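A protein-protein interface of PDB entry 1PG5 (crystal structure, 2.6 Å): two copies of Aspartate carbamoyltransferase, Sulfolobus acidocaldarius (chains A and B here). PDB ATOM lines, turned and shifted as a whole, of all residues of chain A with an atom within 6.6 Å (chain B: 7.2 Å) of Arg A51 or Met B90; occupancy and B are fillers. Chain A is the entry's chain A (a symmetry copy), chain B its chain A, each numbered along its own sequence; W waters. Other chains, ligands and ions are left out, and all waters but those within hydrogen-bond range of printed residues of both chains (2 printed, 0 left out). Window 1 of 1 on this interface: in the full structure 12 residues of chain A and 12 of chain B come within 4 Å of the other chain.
The guanidinium group (NH1) of Arg A262 lies within salt-bridge range of the side-chain carboxylate (OD1) of Asp B86, at 2.6 Å.
NH2 of Arg A51 is in salt-bridge range of OE1 of Glu B82 (2.7 Å).
O of Arg A51 is in hydrogen-bond range of OH of Tyr B94 (2.9 Å).
Printed residues of chain A that touch a printed residue of chain B: Thr A50, Arg A51, Leu A54, Ser A55, Pro A261, Arg A262 and Phe A279.
Of the 18 printed residues of chain B, 6 touch a printed residue of chain A.
Hydrophobic or aromatic side chains of chain B within 4 Å of the printed part of chain A: Phe B70, Met B90 and Tyr B94.
Among the printed residues, 10 pairs touch across the chains.
Among the printed residues, pairs that only touch across the chains: Ser A55 with Tyr B94, Phe A279 with Asp B86, Phe A279 with Arg B89, Leu A54 with Tyr B94, Pro A261 with Glu B82, Arg A51 with Met B90 and Thr A50 with Phe B70.
Water W2 bridges O of Asp B86 (2.4 Å) and NH2 of Arg A51 (2.8 Å).
Water W1 lies within hydrogen-bond range of O of Phe A279 (2.9 Å) and ND2 of Asn B93 (2.9 Å).
Arg A51 touches just these residues of chain B: Glu B82, Met B90 and Tyr B94.
Met B90 touches just one residue of chain A: Arg A51.
Printed residues of chain A within 4 Å of Glu B82: Arg A51 and Pro A261.
Of the printed residues of chain B, Phe A279 touches Asp B86 (3.4 Å) and Arg B89 (3.5 Å).
Of the printed residues of chain A, Asp B86 touches Arg A262 (2.6 Å) and Phe A279 (3.4 Å).
Printed residues of chain A within 4 Å of Arg B89: Phe A279 (3.5 Å).
Of the printed residues of chain B, Thr A50 touches Phe B70.
The nearest residue of chain A that does not touch Met B90 is Leu A54 (4.3 Å).
The nearest printed residue of chain A that does not touch Phe B70 is Leu A54 (4.5 Å).
No position is printed for both chains.
Of the 10 pairs that touch across the chains among the printed residues, none has its exchanged pair printed and touching as well.
The side-chain carboxylate (OE2) of Glu B82 sits at hydrogen-bond distance from the side-chain hydroxyl (OG1) of Thr B87, 2.6 Å away.
The guanidinium group (NH1) of Arg A289 sits at hydrogen-bond distance from the side-chain hydroxyl (OG) of Ser A55, 3.1 Å away.
OD2 of Asp B86 is in salt-bridge range of NH1 of Arg B89.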
ATOM      1  N   PHE A  45      17.929  20.107  -8.313  1.00  0.00           N
ATOM      2  CA  PHE A  45      17.508  19.058  -7.418  1.00  0.00           C
ATOM      3  C   PHE A  45      17.215  19.751  -6.101  1.00  0.00           C
ATOM      4  O   PHE A  45      18.026  19.813  -5.231  1.00  0.00           O
ATOM      5  CB  PHE A  45      18.637  18.056  -7.289  1.00  0.00           C
ATOM      6  CG  PHE A  45      18.544  16.904  -8.254  1.00  0.00           C
ATOM      7  CD1 PHE A  45      18.983  15.653  -7.898  1.00  0.00           C
ATOM      8  CD2 PHE A  45      17.982  17.037  -9.490  1.00  0.00           C
ATOM      9  CE1 PHE A  45      18.876  14.576  -8.788  1.00  0.00           C
ATOM     10  CE2 PHE A  45      17.899  15.940 -10.341  1.00  0.00           C
ATOM     11  CZ  PHE A  45      18.336  14.722  -9.965  1.00  0.00           C
ATOM     12  N   SER A  49      19.642  14.205  -4.446  1.00  0.00           N
ATOM     13  CA  SER A  49      19.975  12.770  -4.583  1.00  0.00           C
ATOM     14  C   SER A  49      21.234  12.705  -5.431  1.00  0.00           C
ATOM     15  O   SER A  49      21.180  12.935  -6.645  1.00  0.00           O
ATOM     16  CB  SER A  49      18.889  12.009  -5.316  1.00  0.00           C
ATOM     17  OG  SER A  49      19.369  10.756  -5.836  1.00  0.00           O
ATOM     18  N   THR A  50      22.349  12.397  -4.836  1.00  0.00           N
ATOM     19  CA  THR A  50      23.597  12.322  -5.542  1.00  0.00           C
ATOM     20  C   THR A  50      23.653  11.259  -6.598  1.00  0.00           C
ATOM     21  O   THR A  50      24.212  11.511  -7.695  1.00  0.00           O
ATOM     22  CB  THR A  50      24.619  12.049  -4.574  1.00  0.00           C
ATOM     23  OG1 THR A  50      24.762  13.220  -3.818  1.00  0.00           O
ATOM     24  CG2 THR A  50      25.976  11.994  -5.202  1.00  0.00           C
ATOM     25  N   ARG A  51      23.093  10.085  -6.288  1.00  0.00           N
ATOM     26  CA  ARG A  51      23.109   8.968  -7.243  1.00  0.00           C
ATOM     27  C   ARG A  51      22.458   9.449  -8.554  1.00  0.00           C
ATOM     28  O   ARG A  51      22.964   9.233  -9.630  1.00  0.00           O
ATOM     29  CB  ARG A  51      22.365   7.766  -6.666  1.00  0.00           C
ATOM     30  CG  ARG A  51      22.095   6.655  -7.663  1.00  0.00           C
ATOM     31  CD  ARG A  51      21.414   5.327  -7.128  1.00  0.00           C
ATOM     32  NE  ARG A  51      22.228   4.602  -6.157  1.00  0.00           N
ATOM     33  CZ  ARG A  51      23.011   3.539  -6.424  1.00  0.00           C
ATOM     34  NH1 ARG A  51      23.138   2.985  -7.653  1.00  0.00           N
ATOM     35  NH2 ARG A  51      23.678   2.990  -5.400  1.00  0.00           N
ATOM     36  N   THR A  52      21.304  10.085  -8.443  1.00  0.00           N
ATOM     37  CA  THR A  52      20.534  10.478  -9.614  1.00  0.00           C
ATOM     38  C   THR A  52      21.082  11.737 -10.220  1.00  0.00           C
ATOM     39  O   THR A  52      21.072  11.862 -11.382  1.00  0.00           O
ATOM     40  CB  THR A  52      19.085  10.717  -9.207  1.00  0.00           C
ATOM     41  OG1 THR A  52      18.601   9.542  -8.544  1.00  0.00           O
ATOM     42  CG2 THR A  52      18.239  10.759 -10.416  1.00  0.00           C
ATOM     43  N   TYR A  53      21.574  12.670  -9.431  1.00  0.00           N
ATOM     44  CA  TYR A  53      22.241  13.829  -9.999  1.00  0.00           C
ATOM     45  C   TYR A  53      23.353  13.368 -10.933  1.00  0.00           C
ATOM     46  O   TYR A  53      23.408  13.737 -12.073  1.00  0.00           O
ATOM     47  CB  TYR A  53      22.741  14.707  -8.872  1.00  0.00           C
ATOM     48  CG  TYR A  53      23.235  16.069  -9.291  1.00  0.00           C
ATOM     49  CD1 TYR A  53      24.438  16.229  -9.988  1.00  0.00           C
ATOM     50  CD2 TYR A  53      22.567  17.193  -8.957  1.00  0.00           C
ATOM     51  CE1 TYR A  53      24.940  17.528 -10.377  1.00  0.00           C
ATOM     52  CE2 TYR A  53      23.047  18.455  -9.302  1.00  0.00           C
ATOM     53  CZ  TYR A  53      24.209  18.627 -10.036  1.00  0.00           C
ATOM     54  OH  TYR A  53      24.622  19.894 -10.347  1.00  0.00           O
ATOM     55  N   LEU A  54      24.164  12.433 -10.490  1.00  0.00           N
ATOM     56  CA  LEU A  54      25.404  12.113 -11.181  1.00  0.00           C
ATOM     57  C   LEU A  54      25.010  11.346 -12.422  1.00  0.00           C
ATOM     58  O   LEU A  54      25.688  11.352 -13.439  1.00  0.00           O
ATOM     59  CB  LEU A  54      26.281  11.247 -10.322  1.00  0.00           C
ATOM     60  CG  LEU A  54      27.433  11.941  -9.636  1.00  0.00           C
ATOM     61  CD1 LEU A  54      27.162  13.258  -9.141  1.00  0.00           C
ATOM     62  CD2 LEU A  54      27.811  11.119  -8.455  1.00  0.00           C
ATOM     63  N   SER A  55      23.907  10.657 -12.329  1.00  0.00           N
ATOM     64  CA  SER A  55      23.532   9.805 -13.409  1.00  0.00           C
ATOM     65  C   SER A  55      23.046  10.689 -14.626  1.00  0.00           C
ATOM     66  O   SER A  55      23.370  10.409 -15.789  1.00  0.00           O
ATOM     67  CB  SER A  55      22.394   8.909 -12.965  1.00  0.00           C
ATOM     68  OG  SER A  55      21.824   8.463 -14.150  1.00  0.00           O
ATOM     69  N   PHE A  56      22.272  11.750 -14.355  1.00  0.00           N
ATOM     70  CA  PHE A  56      21.831  12.601 -15.439  1.00  0.00           C
ATOM     71  C   PHE A  56      23.036  13.420 -15.966  1.00  0.00           C
ATOM     72  O   PHE A  56      23.199  13.577 -17.167  1.00  0.00           O
ATOM     73  CB  PHE A  56      20.780  13.531 -14.951  1.00  0.00           C
ATOM     74  CG  PHE A  56      19.390  12.970 -15.050  1.00  0.00           C
ATOM     75  CD1 PHE A  56      18.738  12.455 -13.943  1.00  0.00           C
ATOM     76  CD2 PHE A  56      18.726  12.957 -16.269  1.00  0.00           C
ATOM     77  CE1 PHE A  56      17.407  11.939 -14.048  1.00  0.00           C
ATOM     78  CE2 PHE A  56      17.448  12.452 -16.365  1.00  0.00           C
ATOM     79  CZ  PHE A  56      16.793  11.951 -15.249  1.00  0.00           C
ATOM     80  N   PRO A 259      15.192  -0.408  -7.187  1.00  0.00           N
ATOM     81  CA  PRO A 259      15.765   0.906  -7.506  1.00  0.00           C
ATOM     82  C   PRO A 259      16.599   1.415  -6.292  1.00  0.00           C
ATOM     83  O   PRO A 259      16.138   1.738  -5.191  1.00  0.00           O
ATOM     84  CB  PRO A 259      14.536   1.750  -7.819  1.00  0.00           C
ATOM     85  CG  PRO A 259      13.499   1.159  -6.903  1.00  0.00           C
ATOM     86  CD  PRO A 259      13.755  -0.307  -6.875  1.00  0.00           C
ATOM     87  N   LEU A 260      17.893   1.440  -6.501  1.00  0.00           N
ATOM     88  CA  LEU A 260      18.836   1.565  -5.410  1.00  0.00           C
ATOM     89  C   LEU A 260      18.801   3.021  -4.864  1.00  0.00           C
ATOM     90  O   LEU A 260      18.314   3.900  -5.546  1.00  0.00           O
ATOM     91  CB  LEU A 260      20.187   1.209  -6.038  1.00  0.00           C
ATOM     92  CG  LEU A 260      21.010  -0.026  -5.630  1.00  0.00           C
ATOM     93  CD1 LEU A 260      20.332  -1.062  -4.700  1.00  0.00           C
ATOM     94  CD2 LEU A 260      21.626  -0.664  -6.895  1.00  0.00           C
ATOM     95  N   PRO A 261      19.341   3.390  -3.717  1.00  0.00           N
ATOM     96  CA  PRO A 261      20.103   2.566  -2.811  1.00  0.00           C
ATOM     97  C   PRO A 261      19.231   1.622  -2.012  1.00  0.00           C
ATOM     98  O   PRO A 261      18.039   1.785  -1.956  1.00  0.00           O
ATOM     99  CB  PRO A 261      20.729   3.633  -1.898  1.00  0.00           C
ATOM    100  CG  PRO A 261      19.721   4.689  -1.867  1.00  0.00           C
ATOM    101  CD  PRO A 261      19.272   4.788  -3.251  1.00  0.00           C
ATOM    102  N   ARG A 262      19.881   0.621  -1.444  1.00  0.00           N
ATOM    103  CA  ARG A 262      19.277  -0.307  -0.518  1.00  0.00           C
ATOM    104  C   ARG A 262      19.880  -0.025   0.846  1.00  0.00           C
ATOM    105  O   ARG A 262      20.880   0.633   0.943  1.00  0.00           O
ATOM    106  CB  ARG A 262      19.499  -1.764  -0.973  1.00  0.00           C
ATOM    107  CG  ARG A 262      20.974  -2.313  -1.089  1.00  0.00           C
ATOM    108  CD  ARG A 262      21.113  -3.744  -0.477  1.00  0.00           C
ATOM    109  NE  ARG A 262      21.727  -4.782  -1.327  1.00  0.00           N
ATOM    110  CZ  ARG A 262      22.975  -4.760  -1.761  1.00  0.00           C
ATOM    111  NH1 ARG A 262      23.775  -3.768  -1.508  1.00  0.00           N
ATOM    112  NH2 ARG A 262      23.443  -5.734  -2.454  1.00  0.00           N
ATOM    113  N   TYR A 278      19.710  -6.095  -9.767  1.00  0.00           N
ATOM    114  CA  TYR A 278      19.569  -4.667  -9.376  1.00  0.00           C
ATOM    115  C   TYR A 278      20.819  -3.856  -9.676  1.00  0.00           C
ATOM    116  O   TYR A 278      20.752  -2.650  -9.904  1.00  0.00           O
ATOM    117  CB  TYR A 278      19.259  -4.479  -7.889  1.00  0.00           C
ATOM    118  CG  TYR A 278      19.701  -5.587  -7.003  1.00  0.00           C
ATOM    119  CD1 TYR A 278      18.848  -6.674  -6.764  1.00  0.00           C
ATOM    120  CD2 TYR A 278      20.955  -5.562  -6.389  1.00  0.00           C
ATOM    121  CE1 TYR A 278      19.224  -7.728  -5.923  1.00  0.00           C
ATOM    122  CE2 TYR A 278      21.368  -6.636  -5.554  1.00  0.00           C
ATOM    123  CZ  TYR A 278      20.496  -7.729  -5.322  1.00  0.00           C
ATOM    124  OH  TYR A 278      20.868  -8.819  -4.513  1.00  0.00           O
ATOM    125  N   PHE A 279      21.956  -4.532  -9.625  1.00  0.00           N
ATOM    126  CA  PHE A 279      23.217  -3.986 -10.067  1.00  0.00           C
ATOM    127  C   PHE A 279      23.206  -3.655 -11.543  1.00  0.00           C
ATOM    128  O   PHE A 279      23.477  -2.545 -11.908  1.00  0.00           O
ATOM    129  CB  PHE A 279      24.388  -4.851  -9.582  1.00  0.00           C
ATOM    130  CG  PHE A 279      24.647  -4.645  -8.091  1.00  0.00           C
ATOM    131  CD1 PHE A 279      24.833  -3.349  -7.584  1.00  0.00           C
ATOM    132  CD2 PHE A 279      24.626  -5.681  -7.190  1.00  0.00           C
ATOM    133  CE1 PHE A 279      25.025  -3.096  -6.232  1.00  0.00           C
ATOM    134  CE2 PHE A 279      24.810  -5.427  -5.842  1.00  0.00           C
ATOM    135  CZ  PHE A 279      25.003  -4.132  -5.369  1.00  0.00           C
ATOM    136  N   ALA A 282      20.832  -0.597 -12.099  1.00  0.00           N
ATOM    137  CA  ALA A 282      21.416   0.738 -11.894  1.00  0.00           C
ATOM    138  C   ALA A 282      22.392   1.090 -13.025  1.00  0.00           C
ATOM    139  O   ALA A 282      22.595   2.222 -13.327  1.00  0.00           O
ATOM    140  CB  ALA A 282      22.065   0.764 -10.557  1.00  0.00           C
ATOM    141  N   ARG A 289      18.885   7.215 -19.870  1.00  0.00           N
ATOM    142  CA  ARG A 289      18.622   8.635 -19.814  1.00  0.00           C
ATOM    143  C   ARG A 289      19.192   9.374 -21.001  1.00  0.00           C
ATOM    144  O   ARG A 289      18.583  10.326 -21.464  1.00  0.00           O
ATOM    145  CB  ARG A 289      19.135   9.230 -18.546  1.00  0.00           C
ATOM    146  CG  ARG A 289      18.226   8.739 -17.477  1.00  0.00           C
ATOM    147  CD  ARG A 289      18.758   8.960 -16.082  1.00  0.00           C
ATOM    148  NE  ARG A 289      17.644   8.734 -15.187  1.00  0.00           N
ATOM    149  CZ  ARG A 289      17.716   8.188 -13.959  1.00  0.00           C
ATOM    150  NH1 ARG A 289      18.828   7.794 -13.448  1.00  0.00           N
ATOM    151  NH2 ARG A 289      16.671   8.035 -13.204  1.00  0.00           N
ATOM    152  N   SER B  42      35.709  10.525 -10.931  1.00  0.00           N
ATOM    153  CA  SER B  42      34.753  11.047  -9.954  1.00  0.00           C
ATOM    154  C   SER B  42      35.502  11.359  -8.677  1.00  0.00           C
ATOM    155  O   SER B  42      36.420  10.651  -8.247  1.00  0.00           O
ATOM    156  CB  SER B  42      33.566  10.076  -9.761  1.00  0.00           C
ATOM    157  OG  SER B  42      34.107   8.920  -9.320  1.00  0.00           O
ATOM    158  N   PHE B  70      31.047  14.510  -5.494  1.00  0.00           N
ATOM    159  CA  PHE B  70      30.179  15.077  -4.462  1.00  0.00           C
ATOM    160  C   PHE B  70      30.991  15.405  -3.262  1.00  0.00           C
ATOM    161  O   PHE B  70      32.130  14.952  -3.122  1.00  0.00           O
ATOM    162  CB  PHE B  70      29.067  14.093  -4.033  1.00  0.00           C
ATOM    163  CG  PHE B  70      29.573  12.760  -3.614  1.00  0.00           C
ATOM    164  CD1 PHE B  70      29.804  12.467  -2.320  1.00  0.00           C
ATOM    165  CD2 PHE B  70      29.778  11.774  -4.517  1.00  0.00           C
ATOM    166  CE1 PHE B  70      30.250  11.218  -1.939  1.00  0.00           C
ATOM    167  CE2 PHE B  70      30.245  10.527  -4.116  1.00  0.00           C
ATOM    168  CZ  PHE B  70      30.479  10.262  -2.845  1.00  0.00           C
ATOM    169  N   GLU B  82      23.456   4.288   3.109  1.00  0.00           N
ATOM    170  CA  GLU B  82      24.152   3.624   2.002  1.00  0.00           C
ATOM    171  C   GLU B  82      25.653   3.341   2.305  1.00  0.00           C
ATOM    172  O   GLU B  82      26.455   4.239   2.517  1.00  0.00           O
ATOM    173  CB  GLU B  82      23.999   4.397   0.664  1.00  0.00           C
ATOM    174  CG  GLU B  82      24.651   3.643  -0.508  1.00  0.00           C
ATOM    175  CD  GLU B  82      24.829   4.350  -1.894  1.00  0.00           C
ATOM    176  OE1 GLU B  82      24.284   3.747  -2.843  1.00  0.00           O
ATOM    177  OE2 GLU B  82      25.557   5.400  -2.129  1.00  0.00           O
ATOM    178  N   ASN B  83      25.950   2.047   2.329  1.00  0.00           N
ATOM    179  CA  ASN B  83      27.233   1.345   2.286  1.00  0.00           C
ATOM    180  C   ASN B  83      28.346   2.003   1.363  1.00  0.00           C
ATOM    181  O   ASN B  83      28.114   2.338   0.208  1.00  0.00           O
ATOM    182  CB  ASN B  83      26.860  -0.138   1.778  1.00  0.00           C
ATOM    183  CG  ASN B  83      28.064  -1.098   1.816  1.00  0.00           C
ATOM    184  OD1 ASN B  83      27.948  -2.271   2.157  1.00  0.00           O
ATOM    185  ND2 ASN B  83      29.295  -0.551   1.519  1.00  0.00           N
ATOM    186  N   LEU B  84      29.568   2.156   1.848  1.00  0.00           N
ATOM    187  CA  LEU B  84      30.690   2.618   0.987  1.00  0.00           C
ATOM    188  C   LEU B  84      30.772   1.703  -0.260  1.00  0.00           C
ATOM    189  O   LEU B  84      30.938   2.198  -1.363  1.00  0.00           O
ATOM    190  CB  LEU B  84      32.014   2.542   1.699  1.00  0.00           C
ATOM    191  CG  LEU B  84      33.191   3.418   1.329  1.00  0.00           C
ATOM    192  CD1 LEU B  84      34.509   2.732   1.646  1.00  0.00           C
ATOM    193  CD2 LEU B  84      33.257   4.007   0.014  1.00  0.00           C
ATOM    194  N   ALA B  85      30.677   0.392  -0.081  1.00  0.00           N
ATOM    195  CA  ALA B  85      30.677  -0.538  -1.214  1.00  0.00           C
ATOM    196  C   ALA B  85      29.613  -0.209  -2.259  1.00  0.00           C
ATOM    197  O   ALA B  85      29.903  -0.292  -3.409  1.00  0.00           O
ATOM    198  CB  ALA B  85      30.554  -1.958  -0.773  1.00  0.00           C
ATOM    199  N   ASP B  86      28.406   0.185  -1.912  1.00  0.00           N
ATOM    200  CA  ASP B  86      27.437   0.471  -2.956  1.00  0.00           C
ATOM    201  C   ASP B  86      27.792   1.738  -3.723  1.00  0.00           C
ATOM    202  O   ASP B  86      27.586   1.833  -4.941  1.00  0.00           O
ATOM    203  CB  ASP B  86      26.052   0.464  -2.351  1.00  0.00           C
ATOM    204  CG  ASP B  86      25.473  -1.020  -2.232  1.00  0.00           C
ATOM    205  OD1 ASP B  86      24.496  -1.298  -1.510  1.00  0.00           O
ATOM    206  OD2 ASP B  86      25.933  -1.998  -2.824  1.00  0.00           O
ATOM    207  N   THR B  87      28.419   2.668  -3.038  1.00  0.00           N
ATOM    208  CA  THR B  87      28.750   3.922  -3.665  1.00  0.00           C
ATOM    209  C   THR B  87      29.869   3.649  -4.606  1.00  0.00           C
ATOM    210  O   THR B  87      29.790   4.089  -5.737  1.00  0.00           O
ATOM    211  CB  THR B  87      29.179   4.990  -2.633  1.00  0.00           C
ATOM    212  OG1 THR B  87      28.078   5.196  -1.779  1.00  0.00           O
ATOM    213  CG2 THR B  87      29.375   6.345  -3.267  1.00  0.00           C
ATOM    214  N   ILE B  88      30.882   2.900  -4.168  1.00  0.00           N
ATOM    215  CA  ILE B  88      31.960   2.533  -5.054  1.00  0.00           C
ATOM    216  C   ILE B  88      31.444   1.834  -6.321  1.00  0.00           C
ATOM    217  O   ILE B  88      31.884   2.163  -7.439  1.00  0.00           O
ATOM    218  CB  ILE B  88      32.954   1.695  -4.370  1.00  0.00           C
ATOM    219  CG1 ILE B  88      33.627   2.459  -3.203  1.00  0.00           C
ATOM    220  CG2 ILE B  88      34.018   1.419  -5.320  1.00  0.00           C
ATOM    221  CD1 ILE B  88      34.166   3.897  -3.456  1.00  0.00           C
ATOM    222  N   ARG B  89      30.490   0.919  -6.151  1.00  0.00           N
ATOM    223  CA  ARG B  89      29.927   0.255  -7.324  1.00  0.00           C
ATOM    224  C   ARG B  89      29.331   1.215  -8.322  1.00  0.00           C
ATOM    225  O   ARG B  89      29.625   1.095  -9.487  1.00  0.00           O
ATOM    226  CB  ARG B  89      28.901  -0.777  -6.998  1.00  0.00           C
ATOM    227  CG  ARG B  89      29.511  -2.041  -6.465  1.00  0.00           C
ATOM    228  CD  ARG B  89      28.523  -3.030  -5.795  1.00  0.00           C
ATOM    229  NE  ARG B  89      29.338  -3.980  -5.071  1.00  0.00           N
ATOM    230  CZ  ARG B  89      29.186  -4.353  -3.795  1.00  0.00           C
ATOM    231  NH1 ARG B  89      28.205  -3.863  -2.990  1.00  0.00           N
ATOM    232  NH2 ARG B  89      30.092  -5.203  -3.311  1.00  0.00           N
ATOM    233  N   MET B  90      28.523   2.155  -7.851  1.00  0.00           N
ATOM    234  CA  MET B  90      27.851   3.154  -8.659  1.00  0.00           C
ATOM    235  C   MET B  90      28.938   3.989  -9.364  1.00  0.00           C
ATOM    236  O   MET B  90      28.874   4.132 -10.572  1.00  0.00           O
ATOM    237  CB  MET B  90      26.892   3.976  -7.766  1.00  0.00           C
ATOM    238  CG  MET B  90      26.514   5.421  -8.245  1.00  0.00           C
ATOM    239  SD  MET B  90      25.874   6.525  -6.868  1.00  0.00           S
ATOM    240  CE  MET B  90      27.286   7.336  -6.420  1.00  0.00           C
ATOM    241  N   LEU B  91      29.969   4.466  -8.664  1.00  0.00           N
ATOM    242  CA  LEU B  91      30.994   5.259  -9.339  1.00  0.00           C
ATOM    243  C   LEU B  91      31.685   4.495 -10.431  1.00  0.00           C
ATOM    244  O   LEU B  91      32.069   5.080 -11.411  1.00  0.00           O
ATOM    245  CB  LEU B  91      32.041   5.866  -8.353  1.00  0.00           C
ATOM    246  CG  LEU B  91      31.400   6.742  -7.265  1.00  0.00           C
ATOM    247  CD1 LEU B  91      32.390   7.127  -6.207  1.00  0.00           C
ATOM    248  CD2 LEU B  91      30.812   7.930  -7.907  1.00  0.00           C
ATOM    249  N   ASN B  92      31.860   3.206 -10.267  1.00  0.00           N
ATOM    250  CA  ASN B  92      32.292   2.341 -11.306  1.00  0.00           C
ATOM    251  C   ASN B  92      31.343   2.340 -12.524  1.00  0.00           C
ATOM    252  O   ASN B  92      31.830   2.317 -13.589  1.00  0.00           O
ATOM    253  CB  ASN B  92      32.487   0.936 -10.785  1.00  0.00           C
ATOM    254  CG  ASN B  92      33.857   0.737 -10.163  1.00  0.00           C
ATOM    255  OD1 ASN B  92      34.108   1.166  -9.007  1.00  0.00           O
ATOM    256  ND2 ASN B  92      34.757   0.133 -10.915  1.00  0.00           N
ATOM    257  N   ASN B  93      30.025   2.410 -12.423  1.00  0.00           N
ATOM    258  CA  ASN B  93      29.236   2.662 -13.655  1.00  0.00           C
ATOM    259  C   ASN B  93      29.572   3.994 -14.256  1.00  0.00           C
ATOM    260  O   ASN B  93      29.597   4.086 -15.423  1.00  0.00           O
ATOM    261  CB  ASN B  93      27.694   2.639 -13.430  1.00  0.00           C
ATOM    262  CG  ASN B  93      27.260   1.357 -12.841  1.00  0.00           C
ATOM    263  OD1 ASN B  93      27.907   0.358 -13.118  1.00  0.00           O
ATOM    264  ND2 ASN B  93      26.250   1.353 -11.940  1.00  0.00           N
ATOM    265  N   TYR B  94      29.792   5.020 -13.451  1.00  0.00           N
ATOM    266  CA  TYR B  94      29.826   6.428 -13.921  1.00  0.00           C
ATOM    267  C   TYR B  94      31.182   6.958 -14.304  1.00  0.00           C
ATOM    268  O   TYR B  94      31.209   8.057 -14.863  1.00  0.00           O
ATOM    269  CB  TYR B  94      29.394   7.429 -12.844  1.00  0.00           C
ATOM    270  CG  TYR B  94      28.022   7.258 -12.378  1.00  0.00           C
ATOM    271  CD1 TYR B  94      27.673   7.741 -11.147  1.00  0.00           C
ATOM    272  CD2 TYR B  94      27.049   6.655 -13.165  1.00  0.00           C
ATOM    273  CE1 TYR B  94      26.367   7.594 -10.637  1.00  0.00           C
ATOM    274  CE2 TYR B  94      25.747   6.481 -12.692  1.00  0.00           C
ATOM    275  CZ  TYR B  94      25.407   6.963 -11.402  1.00  0.00           C
ATOM    276  OH  TYR B  94      24.164   6.900 -10.841  1.00  0.00           O
ATOM    277  N   SER B  95      32.271   6.266 -13.975  1.00  0.00           N
ATOM    278  CA  SER B  95      33.529   6.901 -14.108  1.00  0.00           C
ATOM    279  C   SER B  95      34.642   5.933 -14.338  1.00  0.00           C
ATOM    280  O   SER B  95      34.440   4.733 -14.279  1.00  0.00           O
ATOM    281  CB  SER B  95      33.757   7.840 -12.913  1.00  0.00           C
ATOM    282  OG  SER B  95      34.038   7.221 -11.670  1.00  0.00           O
ATOM    283  N   ILE B  98      38.448   6.978  -9.276  1.00  0.00           N
ATOM    284  CA  ILE B  98      37.814   7.636  -8.155  1.00  0.00           C
ATOM    285  C   ILE B  98      38.854   8.312  -7.256  1.00  0.00           C
ATOM    286  O   ILE B  98      39.779   7.703  -6.889  1.00  0.00           O
ATOM    287  CB  ILE B  98      37.118   6.546  -7.337  1.00  0.00           C
ATOM    288  CG1 ILE B  98      35.971   5.890  -8.110  1.00  0.00           C
ATOM    289  CG2 ILE B  98      36.619   7.123  -6.042  1.00  0.00           C
ATOM    290  CD1 ILE B  98      35.380   4.572  -7.469  1.00  0.00           C
ATOM    291  N   ILE B 117      37.994   0.351 -11.449  1.00  0.00           N
ATOM    292  CA  ILE B 117      38.752   1.537 -11.807  1.00  0.00           C
ATOM    293  C   ILE B 117      39.667   1.923 -10.624  1.00  0.00           C
ATOM    294  O   ILE B 117      39.432   1.519  -9.453  1.00  0.00           O
ATOM    295  CB  ILE B 117      37.814   2.618 -12.205  1.00  0.00           C
ATOM    296  CG1 ILE B 117      37.056   3.192 -10.974  1.00  0.00           C
ATOM    297  CG2 ILE B 117      36.886   2.090 -13.389  1.00  0.00           C
ATOM    298  CD1 ILE B 117      35.842   4.098 -11.366  1.00  0.00           C
HETATM  299  O   HOH W   1      25.529  -1.087 -10.494  1.00  0.00           O
HETATM  300  O   HOH W   2      25.525   0.999  -5.897  1.00  0.00           O
